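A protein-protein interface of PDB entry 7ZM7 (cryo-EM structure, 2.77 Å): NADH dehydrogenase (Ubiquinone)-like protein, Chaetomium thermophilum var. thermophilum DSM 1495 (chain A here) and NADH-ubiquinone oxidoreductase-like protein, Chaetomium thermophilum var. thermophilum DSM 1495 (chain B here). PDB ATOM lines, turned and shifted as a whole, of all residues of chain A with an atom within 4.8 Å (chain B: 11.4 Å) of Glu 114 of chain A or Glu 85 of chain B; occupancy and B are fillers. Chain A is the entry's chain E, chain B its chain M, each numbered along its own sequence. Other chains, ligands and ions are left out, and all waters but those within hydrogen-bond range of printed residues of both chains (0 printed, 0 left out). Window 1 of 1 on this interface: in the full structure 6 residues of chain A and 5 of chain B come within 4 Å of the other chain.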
ATOM      1  N   MET A 102      11.209  -5.493  11.611  1.00  0.00           N
ATOM      2  CA  MET A 102      10.051  -5.815  12.423  1.00  0.00           C
ATOM      3  C   MET A 102      10.340  -5.427  13.861  1.00  0.00           C
ATOM      4  O   MET A 102      11.429  -5.690  14.370  1.00  0.00           O
ATOM      5  CB  MET A 102       9.735  -7.300  12.366  1.00  0.00           C
ATOM      6  CG  MET A 102       9.160  -7.765  11.073  1.00  0.00           C
ATOM      7  SD  MET A 102       7.384  -7.690  10.978  1.00  0.00           S
ATOM      8  CE  MET A 102       7.194  -6.441   9.732  1.00  0.00           C
ATOM      9  N   GLU A 103       9.368  -4.744  14.473  1.00  0.00           N
ATOM     10  CA  GLU A 103       9.473  -4.334  15.894  1.00  0.00           C
ATOM     11  C   GLU A 103       9.101  -5.554  16.735  1.00  0.00           C
ATOM     12  O   GLU A 103       7.980  -6.065  16.564  1.00  0.00           O
ATOM     13  CB  GLU A 103       8.515  -3.160  16.099  1.00  0.00           C
ATOM     14  CG  GLU A 103       8.201  -2.830  17.544  1.00  0.00           C
ATOM     15  CD  GLU A 103       7.090  -1.801  17.663  1.00  0.00           C
ATOM     16  OE1 GLU A 103       6.567  -1.384  16.613  1.00  0.00           O
ATOM     17  OE2 GLU A 103       6.752  -1.421  18.795  1.00  0.00           O
ATOM     18  N   GLN A 110       3.537 -12.853  19.462  1.00  0.00           N
ATOM     19  CA  GLN A 110       3.006 -12.496  18.157  1.00  0.00           C
ATOM     20  C   GLN A 110       4.079 -11.870  17.284  1.00  0.00           C
ATOM     21  O   GLN A 110       4.226 -12.230  16.114  1.00  0.00           O
ATOM     22  CB  GLN A 110       1.827 -11.542  18.327  1.00  0.00           C
ATOM     23  CG  GLN A 110       1.264 -10.894  17.061  1.00  0.00           C
ATOM     24  CD  GLN A 110       1.264 -11.783  15.828  1.00  0.00           C
ATOM     25  OE1 GLN A 110       1.154 -13.005  15.911  1.00  0.00           O
ATOM     26  NE2 GLN A 110       1.363 -11.157  14.667  1.00  0.00           N
ATOM     27  N   SER A 111       4.854 -10.949  17.844  1.00  0.00           N
ATOM     28  CA  SER A 111       5.984 -10.334  17.102  1.00  0.00           C
ATOM     29  C   SER A 111       6.932 -11.430  16.600  1.00  0.00           C
ATOM     30  O   SER A 111       7.393 -11.331  15.464  1.00  0.00           O
ATOM     31  CB  SER A 111       6.693  -9.340  17.975  1.00  0.00           C
ATOM     32  OG  SER A 111       7.284  -9.970  19.096  1.00  0.00           O
ATOM     33  N   ILE A 112       7.270 -12.393  17.453  1.00  0.00           N
ATOM     34  CA  ILE A 112       8.110 -13.551  17.030  1.00  0.00           C
ATOM     35  C   ILE A 112       7.344 -14.390  16.009  1.00  0.00           C
ATOM     36  O   ILE A 112       7.958 -14.792  15.011  1.00  0.00           O
ATOM     37  CB  ILE A 112       8.574 -14.368  18.253  1.00  0.00           C
ATOM     38  CG1 ILE A 112       9.457 -13.506  19.158  1.00  0.00           C
ATOM     39  CG2 ILE A 112       9.268 -15.652  17.840  1.00  0.00           C
ATOM     40  CD1 ILE A 112       9.908 -14.189  20.418  1.00  0.00           C
ATOM     41  N   GLU A 113       6.054 -14.634  16.233  1.00  0.00           N
ATOM     42  CA  GLU A 113       5.376 -15.525  15.305  1.00  0.00           C
ATOM     43  C   GLU A 113       5.420 -14.959  13.900  1.00  0.00           C
ATOM     44  O   GLU A 113       5.909 -15.609  12.973  1.00  0.00           O
ATOM     45  CB  GLU A 113       3.939 -15.767  15.747  1.00  0.00           C
ATOM     46  CG  GLU A 113       3.860 -16.510  17.049  1.00  0.00           C
ATOM     47  CD  GLU A 113       4.388 -17.918  16.950  1.00  0.00           C
ATOM     48  OE1 GLU A 113       4.270 -18.530  15.879  1.00  0.00           O
ATOM     49  OE2 GLU A 113       4.923 -18.425  17.953  1.00  0.00           O
ATOM     50  N   GLU A 114       4.987 -13.714  13.742  1.00  0.00           N
ATOM     51  CA  GLU A 114       4.894 -13.098  12.432  1.00  0.00           C
ATOM     52  C   GLU A 114       6.250 -12.724  11.849  1.00  0.00           C
ATOM     53  O   GLU A 114       6.305 -12.299  10.696  1.00  0.00           O
ATOM     54  CB  GLU A 114       3.971 -11.882  12.510  1.00  0.00           C
ATOM     55  CG  GLU A 114       4.411 -10.802  13.459  1.00  0.00           C
ATOM     56  CD  GLU A 114       5.326  -9.807  12.807  1.00  0.00           C
ATOM     57  OE1 GLU A 114       5.287  -9.724  11.575  1.00  0.00           O
ATOM     58  OE2 GLU A 114       6.107  -9.139  13.515  1.00  0.00           O
ATOM     59  N   SER A 115       7.339 -12.858  12.605  1.00  0.00           N
ATOM     60  CA  SER A 115       8.651 -12.641  12.008  1.00  0.00           C
ATOM     61  C   SER A 115       9.162 -13.867  11.264  1.00  0.00           C
ATOM     62  O   SER A 115      10.013 -13.733  10.383  1.00  0.00           O
ATOM     63  CB  SER A 115       9.666 -12.225  13.070  1.00  0.00           C
ATOM     64  OG  SER A 115       9.539 -10.852  13.376  1.00  0.00           O
ATOM     65  N   VAL A 116       8.648 -15.055  11.575  1.00  0.00           N
ATOM     66  CA  VAL A 116       9.188 -16.298  11.043  1.00  0.00           C
ATOM     67  C   VAL A 116       8.204 -17.051  10.167  1.00  0.00           C
ATOM     68  O   VAL A 116       8.506 -18.179   9.768  1.00  0.00           O
ATOM     69  CB  VAL A 116       9.702 -17.219  12.166  1.00  0.00           C
ATOM     70  CG1 VAL A 116      10.693 -16.518  13.021  1.00  0.00           C
ATOM     71  CG2 VAL A 116       8.562 -17.726  12.993  1.00  0.00           C
ATOM     72  N   ARG A 117       7.047 -16.473   9.833  1.00  0.00           N
ATOM     73  CA  ARG A 117       6.058 -17.246   9.084  1.00  0.00           C
ATOM     74  C   ARG A 117       6.456 -17.449   7.632  1.00  0.00           C
ATOM     75  O   ARG A 117       5.969 -18.379   6.988  1.00  0.00           O
ATOM     76  CB  ARG A 117       4.682 -16.595   9.138  1.00  0.00           C
ATOM     77  CG  ARG A 117       4.308 -16.042  10.473  1.00  0.00           C
ATOM     78  CD  ARG A 117       2.819 -15.699  10.578  1.00  0.00           C
ATOM     79  NE  ARG A 117       2.422 -14.548   9.780  1.00  0.00           N
ATOM     80  CZ  ARG A 117       1.988 -14.623   8.527  1.00  0.00           C
ATOM     81  NH1 ARG A 117       1.872 -15.797   7.925  1.00  0.00           N
ATOM     82  NH2 ARG A 117       1.646 -13.524   7.875  1.00  0.00           N
ATOM     83  N   HIS A 118       7.319 -16.598   7.098  1.00  0.00           N
ATOM     84  CA  HIS A 118       7.707 -16.657   5.700  1.00  0.00           C
ATOM     85  C   HIS A 118       9.126 -17.157   5.517  1.00  0.00           C
ATOM     86  O   HIS A 118       9.531 -17.446   4.386  1.00  0.00           O
ATOM     87  CB  HIS A 118       7.557 -15.276   5.060  1.00  0.00           C
ATOM     88  CG  HIS A 118       6.221 -14.649   5.295  1.00  0.00           C
ATOM     89  ND1 HIS A 118       5.105 -14.978   4.562  1.00  0.00           N
ATOM     90  CD2 HIS A 118       5.818 -13.724   6.194  1.00  0.00           C
ATOM     91  CE1 HIS A 118       4.074 -14.280   4.993  1.00  0.00           C
ATOM     92  NE2 HIS A 118       4.480 -13.509   5.981  1.00  0.00           N
ATOM     93  N   THR B  51      -1.875 -10.580   6.519  1.00  0.00           N
ATOM     94  CA  THR B  51      -2.758 -10.761   5.376  1.00  0.00           C
ATOM     95  C   THR B  51      -3.886 -11.738   5.679  1.00  0.00           C
ATOM     96  O   THR B  51      -3.919 -12.360   6.740  1.00  0.00           O
ATOM     97  CB  THR B  51      -1.992 -11.268   4.152  1.00  0.00           C
ATOM     98  OG1 THR B  51      -2.912 -11.500   3.079  1.00  0.00           O
ATOM     99  CG2 THR B  51      -1.273 -12.565   4.476  1.00  0.00           C
ATOM    100  N   GLY B  52      -4.811 -11.866   4.740  1.00  0.00           N
ATOM    101  CA  GLY B  52      -5.904 -12.825   4.886  1.00  0.00           C
ATOM    102  C   GLY B  52      -7.041 -12.431   5.795  1.00  0.00           C
ATOM    103  O   GLY B  52      -8.203 -12.466   5.384  1.00  0.00           O
ATOM    104  N   ARG B  53      -6.739 -12.066   7.040  1.00  0.00           N
ATOM    105  CA  ARG B  53      -7.803 -11.723   7.981  1.00  0.00           C
ATOM    106  C   ARG B  53      -8.610 -10.506   7.550  1.00  0.00           C
ATOM    107  O   ARG B  53      -9.849 -10.596   7.525  1.00  0.00           O
ATOM    108  CB  ARG B  53      -7.207 -11.546   9.382  1.00  0.00           C
ATOM    109  CG  ARG B  53      -6.217 -12.631   9.771  1.00  0.00           C
ATOM    110  CD  ARG B  53      -6.921 -13.872  10.307  1.00  0.00           C
ATOM    111  NE  ARG B  53      -7.549 -14.657   9.246  1.00  0.00           N
ATOM    112  CZ  ARG B  53      -6.886 -15.417   8.379  1.00  0.00           C
ATOM    113  NH1 ARG B  53      -5.564 -15.507   8.440  1.00  0.00           N
ATOM    114  NH2 ARG B  53      -7.549 -16.092   7.450  1.00  0.00           N
ATOM    115  N   PRO B  54      -8.014  -9.364   7.205  1.00  0.00           N
ATOM    116  CA  PRO B  54      -8.834  -8.228   6.777  1.00  0.00           C
ATOM    117  C   PRO B  54      -9.475  -8.488   5.426  1.00  0.00           C
ATOM    118  O   PRO B  54      -8.946  -9.222   4.590  1.00  0.00           O
ATOM    119  CB  PRO B  54      -7.832  -7.068   6.704  1.00  0.00           C
ATOM    120  CG  PRO B  54      -6.613  -7.546   7.417  1.00  0.00           C
ATOM    121  CD  PRO B  54      -6.585  -9.014   7.198  1.00  0.00           C
ATOM    122  N   ALA B  57      -7.497  -6.784   2.339  1.00  0.00           N
ATOM    123  CA  ALA B  57      -6.396  -7.570   1.813  1.00  0.00           C
ATOM    124  C   ALA B  57      -6.852  -8.724   0.926  1.00  0.00           C
ATOM    125  O   ALA B  57      -6.012  -9.362   0.289  1.00  0.00           O
ATOM    126  CB  ALA B  57      -5.552  -8.112   2.965  1.00  0.00           C
ATOM    127  N   ARG B  75      -4.977  -9.433  -5.140  1.00  0.00           N
ATOM    128  CA  ARG B  75      -4.437  -8.772  -3.958  1.00  0.00           C
ATOM    129  C   ARG B  75      -4.055  -9.772  -2.882  1.00  0.00           C
ATOM    130  O   ARG B  75      -3.200  -9.486  -2.043  1.00  0.00           O
ATOM    131  CB  ARG B  75      -5.434  -7.794  -3.356  1.00  0.00           C
ATOM    132  CG  ARG B  75      -5.847  -6.669  -4.201  1.00  0.00           C
ATOM    133  CD  ARG B  75      -6.704  -5.769  -3.377  1.00  0.00           C
ATOM    134  NE  ARG B  75      -5.906  -5.016  -2.429  1.00  0.00           N
ATOM    135  CZ  ARG B  75      -5.433  -3.804  -2.679  1.00  0.00           C
ATOM    136  NH1 ARG B  75      -4.715  -3.171  -1.775  1.00  0.00           N
ATOM    137  NH2 ARG B  75      -5.693  -3.221  -3.833  1.00  0.00           N
ATOM    138  N   SER B  76      -4.714 -10.924  -2.863  1.00  0.00           N
ATOM    139  CA  SER B  76      -4.359 -11.969  -1.923  1.00  0.00           C
ATOM    140  C   SER B  76      -2.927 -12.434  -2.136  1.00  0.00           C
ATOM    141  O   SER B  76      -2.210 -12.722  -1.175  1.00  0.00           O
ATOM    142  CB  SER B  76      -5.334 -13.127  -2.075  1.00  0.00           C
ATOM    143  OG  SER B  76      -6.639 -12.715  -1.728  1.00  0.00           O
ATOM    144  N   GLU B  77      -2.493 -12.512  -3.387  1.00  0.00           N
ATOM    145  CA  GLU B  77      -1.143 -12.978  -3.663  1.00  0.00           C
ATOM    146  C   GLU B  77      -0.150 -11.831  -3.717  1.00  0.00           C
ATOM    147  O   GLU B  77       1.043 -12.040  -3.489  1.00  0.00           O
ATOM    148  CB  GLU B  77      -1.129 -13.762  -4.969  1.00  0.00           C
ATOM    149  CG  GLU B  77      -1.921 -15.036  -4.887  1.00  0.00           C
ATOM    150  CD  GLU B  77      -1.304 -16.043  -3.928  1.00  0.00           C
ATOM    151  OE1 GLU B  77      -0.061 -16.065  -3.791  1.00  0.00           O
ATOM    152  OE2 GLU B  77      -2.067 -16.802  -3.296  1.00  0.00           O
ATOM    153  N   ALA B  78      -0.623 -10.624  -4.025  1.00  0.00           N
ATOM    154  CA  ALA B  78       0.250  -9.461  -4.077  1.00  0.00           C
ATOM    155  C   ALA B  78       0.618  -8.981  -2.693  1.00  0.00           C
ATOM    156  O   ALA B  78       1.709  -8.441  -2.493  1.00  0.00           O
ATOM    157  CB  ALA B  78      -0.426  -8.338  -4.842  1.00  0.00           C
ATOM    158  N   MET B  79      -0.282  -9.163  -1.733  1.00  0.00           N
ATOM    159  CA  MET B  79      -0.115  -8.691  -0.370  1.00  0.00           C
ATOM    160  C   MET B  79       0.082  -9.847   0.593  1.00  0.00           C
ATOM    161  O   MET B  79      -0.356  -9.783   1.743  1.00  0.00           O
ATOM    162  CB  MET B  79      -1.311  -7.828   0.034  1.00  0.00           C
ATOM    163  CG  MET B  79      -1.596  -6.715  -0.952  1.00  0.00           C
ATOM    164  SD  MET B  79      -3.003  -5.701  -0.491  1.00  0.00           S
ATOM    165  CE  MET B  79      -2.189  -4.227   0.074  1.00  0.00           C
ATOM    166  N   ALA B  80       0.691 -10.924   0.123  1.00  0.00           N
ATOM    167  CA  ALA B  80       1.248 -11.954   0.982  1.00  0.00           C
ATOM    168  C   ALA B  80       2.744 -11.717   1.122  1.00  0.00           C
ATOM    169  O   ALA B  80       3.347 -10.978   0.347  1.00  0.00           O
ATOM    170  CB  ALA B  80       0.974 -13.344   0.415  1.00  0.00           C
ATOM    171  N   GLY B  81       3.339 -12.318   2.135  1.00  0.00           N
ATOM    172  CA  GLY B  81       4.769 -12.216   2.303  1.00  0.00           C
ATOM    173  C   GLY B  81       5.202 -11.354   3.470  1.00  0.00           C
ATOM    174  O   GLY B  81       4.390 -10.762   4.183  1.00  0.00           O
ATOM    175  N   PRO B  82       6.516 -11.256   3.668  1.00  0.00           N
ATOM    176  CA  PRO B  82       7.021 -10.573   4.865  1.00  0.00           C
ATOM    177  C   PRO B  82       6.776  -9.072   4.885  1.00  0.00           C
ATOM    178  O   PRO B  82       6.561  -8.517   5.967  1.00  0.00           O
ATOM    179  CB  PRO B  82       8.520 -10.902   4.840  1.00  0.00           C
ATOM    180  CG  PRO B  82       8.675 -11.965   3.854  1.00  0.00           C
ATOM    181  CD  PRO B  82       7.605 -11.802   2.859  1.00  0.00           C
ATOM    182  N   ARG B  83       6.799  -8.390   3.738  1.00  0.00           N
ATOM    183  CA  ARG B  83       6.666  -6.936   3.759  1.00  0.00           C
ATOM    184  C   ARG B  83       5.305  -6.479   4.265  1.00  0.00           C
ATOM    185  O   ARG B  83       5.170  -5.328   4.680  1.00  0.00           O
ATOM    186  CB  ARG B  83       6.914  -6.330   2.373  1.00  0.00           C
ATOM    187  CG  ARG B  83       8.326  -6.442   1.861  1.00  0.00           C
ATOM    188  CD  ARG B  83       8.564  -5.629   0.574  1.00  0.00           C
ATOM    189  NE  ARG B  83       7.709  -6.025  -0.548  1.00  0.00           N
ATOM    190  CZ  ARG B  83       6.718  -5.286  -1.036  1.00  0.00           C
ATOM    191  NH1 ARG B  83       6.001  -5.728  -2.046  1.00  0.00           N
ATOM    192  NH2 ARG B  83       6.426  -4.115  -0.503  1.00  0.00           N
ATOM    193  N   PHE B  84       4.294  -7.339   4.230  1.00  0.00           N
ATOM    194  CA  PHE B  84       2.947  -6.949   4.602  1.00  0.00           C
ATOM    195  C   PHE B  84       2.569  -7.436   5.992  1.00  0.00           C
ATOM    196  O   PHE B  84       1.385  -7.487   6.328  1.00  0.00           O
ATOM    197  CB  PHE B  84       1.963  -7.434   3.541  1.00  0.00           C
ATOM    198  CG  PHE B  84       2.114  -6.721   2.238  1.00  0.00           C
ATOM    199  CD1 PHE B  84       1.466  -5.527   2.007  1.00  0.00           C
ATOM    200  CD2 PHE B  84       2.932  -7.225   1.251  1.00  0.00           C
ATOM    201  CE1 PHE B  84       1.629  -4.857   0.828  1.00  0.00           C
ATOM    202  CE2 PHE B  84       3.094  -6.557   0.057  1.00  0.00           C
ATOM    203  CZ  PHE B  84       2.441  -5.371  -0.153  1.00  0.00           C
ATOM    204  N   GLU B  85       3.561  -7.802   6.797  1.00  0.00           N
ATOM    205  CA  GLU B  85       3.418  -8.065   8.219  1.00  0.00           C
ATOM    206  C   GLU B  85       3.578  -6.759   8.971  1.00  0.00           C
ATOM    207  O   GLU B  85       4.289  -5.858   8.518  1.00  0.00           O
ATOM    208  CB  GLU B  85       4.480  -9.035   8.712  1.00  0.00           C
ATOM    209  CG  GLU B  85       4.659 -10.253   7.880  1.00  0.00           C
ATOM    210  CD  GLU B  85       3.470 -11.150   7.942  1.00  0.00           C
ATOM    211  OE1 GLU B  85       2.800 -11.166   8.995  1.00  0.00           O
ATOM    212  OE2 GLU B  85       3.191 -11.837   6.939  1.00  0.00           O
ATOM    213  N   GLN B  86       2.934  -6.670  10.131  1.00  0.00           N
ATOM    214  CA  GLN B  86       2.981  -5.472  10.959  1.00  0.00           C
ATOM    215  C   GLN B  86       2.486  -4.272  10.166  1.00  0.00           C
ATOM    216  O   GLN B  86       3.098  -3.207  10.143  1.00  0.00           O
ATOM    217  CB  GLN B  86       4.385  -5.237  11.506  1.00  0.00           C
ATOM    218  CG  GLN B  86       4.715  -6.049  12.724  1.00  0.00           C
ATOM    219  CD  GLN B  86       5.910  -5.518  13.448  1.00  0.00           C
ATOM    220  OE1 GLN B  86       6.811  -4.954  12.843  1.00  0.00           O
ATOM    221  NE2 GLN B  86       5.929  -5.692  14.753  1.00  0.00           N
ATOM    222  N   THR B  87       1.345  -4.466   9.519  1.00  0.00           N
ATOM    223  CA  THR B  87       0.836  -3.573   8.496  1.00  0.00           C
ATOM    224  C   THR B  87      -0.653  -3.348   8.702  1.00  0.00           C
ATOM    225  O   THR B  87      -1.382  -4.243   9.123  1.00  0.00           O
ATOM    226  CB  THR B  87       1.098  -4.165   7.107  1.00  0.00           C
ATOM    227  OG1 THR B  87       2.504  -4.333   6.927  1.00  0.00           O
ATOM    228  CG2 THR B  87       0.539  -3.283   6.007  1.00  0.00           C
ATOM    229  N   ASP B  88      -1.093  -2.137   8.387  1.00  0.00           N
ATOM    230  CA  ASP B  88      -2.506  -1.789   8.326  1.00  0.00           C
ATOM    231  C   ASP B  88      -2.973  -1.932   6.882  1.00  0.00           C
ATOM    232  O   ASP B  88      -2.529  -1.189   6.004  1.00  0.00           O
ATOM    233  CB  ASP B  88      -2.733  -0.373   8.838  1.00  0.00           C
ATOM    234  CG  ASP B  88      -4.190  -0.015   8.897  1.00  0.00           C
ATOM    235  OD1 ASP B  88      -5.027  -0.938   8.876  1.00  0.00           O
ATOM    236  OD2 ASP B  88      -4.514   1.189   8.968  1.00  0.00           O
ATOM    237  N   PHE B  89      -3.875  -2.883   6.639  1.00  0.00           N
ATOM    238  CA  PHE B  89      -4.399  -3.115   5.302  1.00  0.00           C
ATOM    239  C   PHE B  89      -5.565  -2.214   4.964  1.00  0.00           C
ATOM    240  O   PHE B  89      -5.960  -2.148   3.802  1.00  0.00           O
ATOM    241  CB  PHE B  89      -4.836  -4.567   5.147  1.00  0.00           C
ATOM    242  CG  PHE B  89      -3.703  -5.511   5.010  1.00  0.00           C
ATOM    243  CD1 PHE B  89      -2.858  -5.446   3.920  1.00  0.00           C
ATOM    244  CD2 PHE B  89      -3.466  -6.461   5.973  1.00  0.00           C
ATOM    245  CE1 PHE B  89      -1.801  -6.318   3.807  1.00  0.00           C
ATOM    246  CE2 PHE B  89      -2.419  -7.333   5.855  1.00  0.00           C
ATOM    247  CZ  PHE B  89      -1.589  -7.267   4.776  1.00  0.00           C
ATOM    248  N   GLN B  92      -4.110   0.785   3.182  1.00  0.00           N
ATOM    249  CA  GLN B  92      -3.491   0.516   1.871  1.00  0.00           C
ATOM    250  C   GLN B  92      -4.326   1.157   0.764  1.00  0.00           C
ATOM    251  O   GLN B  92      -5.555   1.142   0.877  1.00  0.00           O
ATOM    252  CB  GLN B  92      -3.199  -0.981   1.778  1.00  0.00           C
ATOM    253  CG  GLN B  92      -2.089  -1.429   2.715  1.00  0.00           C
ATOM    254  CD  GLN B  92      -0.859  -0.562   2.614  1.00  0.00           C
ATOM    255  OE1 GLN B  92      -0.338  -0.311   1.530  1.00  0.00           O
ATOM    256  NE2 GLN B  92      -0.382  -0.099   3.757  1.00  0.00           N
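The side-chain hydroxyl (OG1) of Thr 87 of chain B is in hydrogen-bond range of the backbone carbonyl oxygen (O) of Glu 85 of chain B (2.8 Å). A ring nitrogen (NE2) of His 118 of chain A sits at hydrogen-bond distance from the guanidinium group (NH2) of Arg 117 of chain A, at 3.4 Å.
O of Glu 103 of chain A is in hydrogen-bond range of NE2 of Gln 86 of chain B, at 2.8 Å. A ring nitrogen (NE2) of His 118 of chain A sits at hydrogen-bond distance from the backbone carbonyl oxygen (O) of Gly 81 of chain B, 3.3 Å away. The side-chain carboxylate of Glu 85 of chain B lies within salt-bridge range of the guanidinium group of Arg 117 of chain A, 2.5 Å away. A ring nitrogen (NE2) of His 118 of chain A lies close to the side-chain carboxylate (OE2) of Glu 85 of chain B (2.3 Å). SD of Met 102 of chain A sits close to OE1 of Gln 86 of chain B.
Hydrophobic or aromatic side chains of chain B within 4 Å of the printed part of chain A: Pro 82. Of the 11 printed residues of chain A, 5 touch a printed residue of chain B. Printed residues of chain A that touch a printed residue of chain B: Met 102, Glu 103, Glu 114, Arg 117 and His 118. Among the printed residues, 9 pairs touch across the chains. Among the printed residues, Asp or Glu carboxylates within 4 Å of a Lys or Arg side-chain nitrogen of the other chain: Arg 117 of chain A with Glu 85 of chain B (2.5 Å).
Among the printed residues, pairs that only touch across the chains: Met 102 of chain A with Glu 85 of chain B (3.2 Å), Glu 114 of chain A with Glu 85 of chain B (3.1 Å), Glu 114 of chain A with Gln 86 of chain B (3.5 Å) and His 118 of chain A with Pro 82 of chain B (3.6 Å).
Glu 114 of chain A touches just these residues of chain B: Glu 85 (3.1 Å) and Gln 86 (3.5 Å). Glu 85 of chain B touches just these residues of chain A: Met 102 (3.2 Å), Glu 114 (3.1 Å), Arg 117 (2.5 Å) and His 118 (2.3 Å). No residue of chain B comes within 4 Å of Glu 113 of chain A. No residue of chain B comes within 4 Å of Ser 115 of chain A. Printed residues of chain B within 4 Å of His 118 of chain A: Gly 81, Pro 82 and Glu 85. Printed residues of chain A within 4 Å of Gly 81 of chain B: His 118. Printed residues of chain B within 4 Å of Glu 103 of chain A: Gln 86. Printed residues of chain A within 4 Å of Gln 86 of chain B: Met 102 (3.4 Å), Glu 103 (2.8 Å) and Glu 114 (3.5 Å). Of the printed residues of chain A, Pro 82 of chain B touches His 118 (3.6 Å). The nearest printed residue of chain A that does not touch Glu 85 of chain B is Gln 110 of chain A (5.9 Å). The nearest printed residue of chain A that does not touch Gln 86 of chain B is Ser 111 of chain A (4.9 Å).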
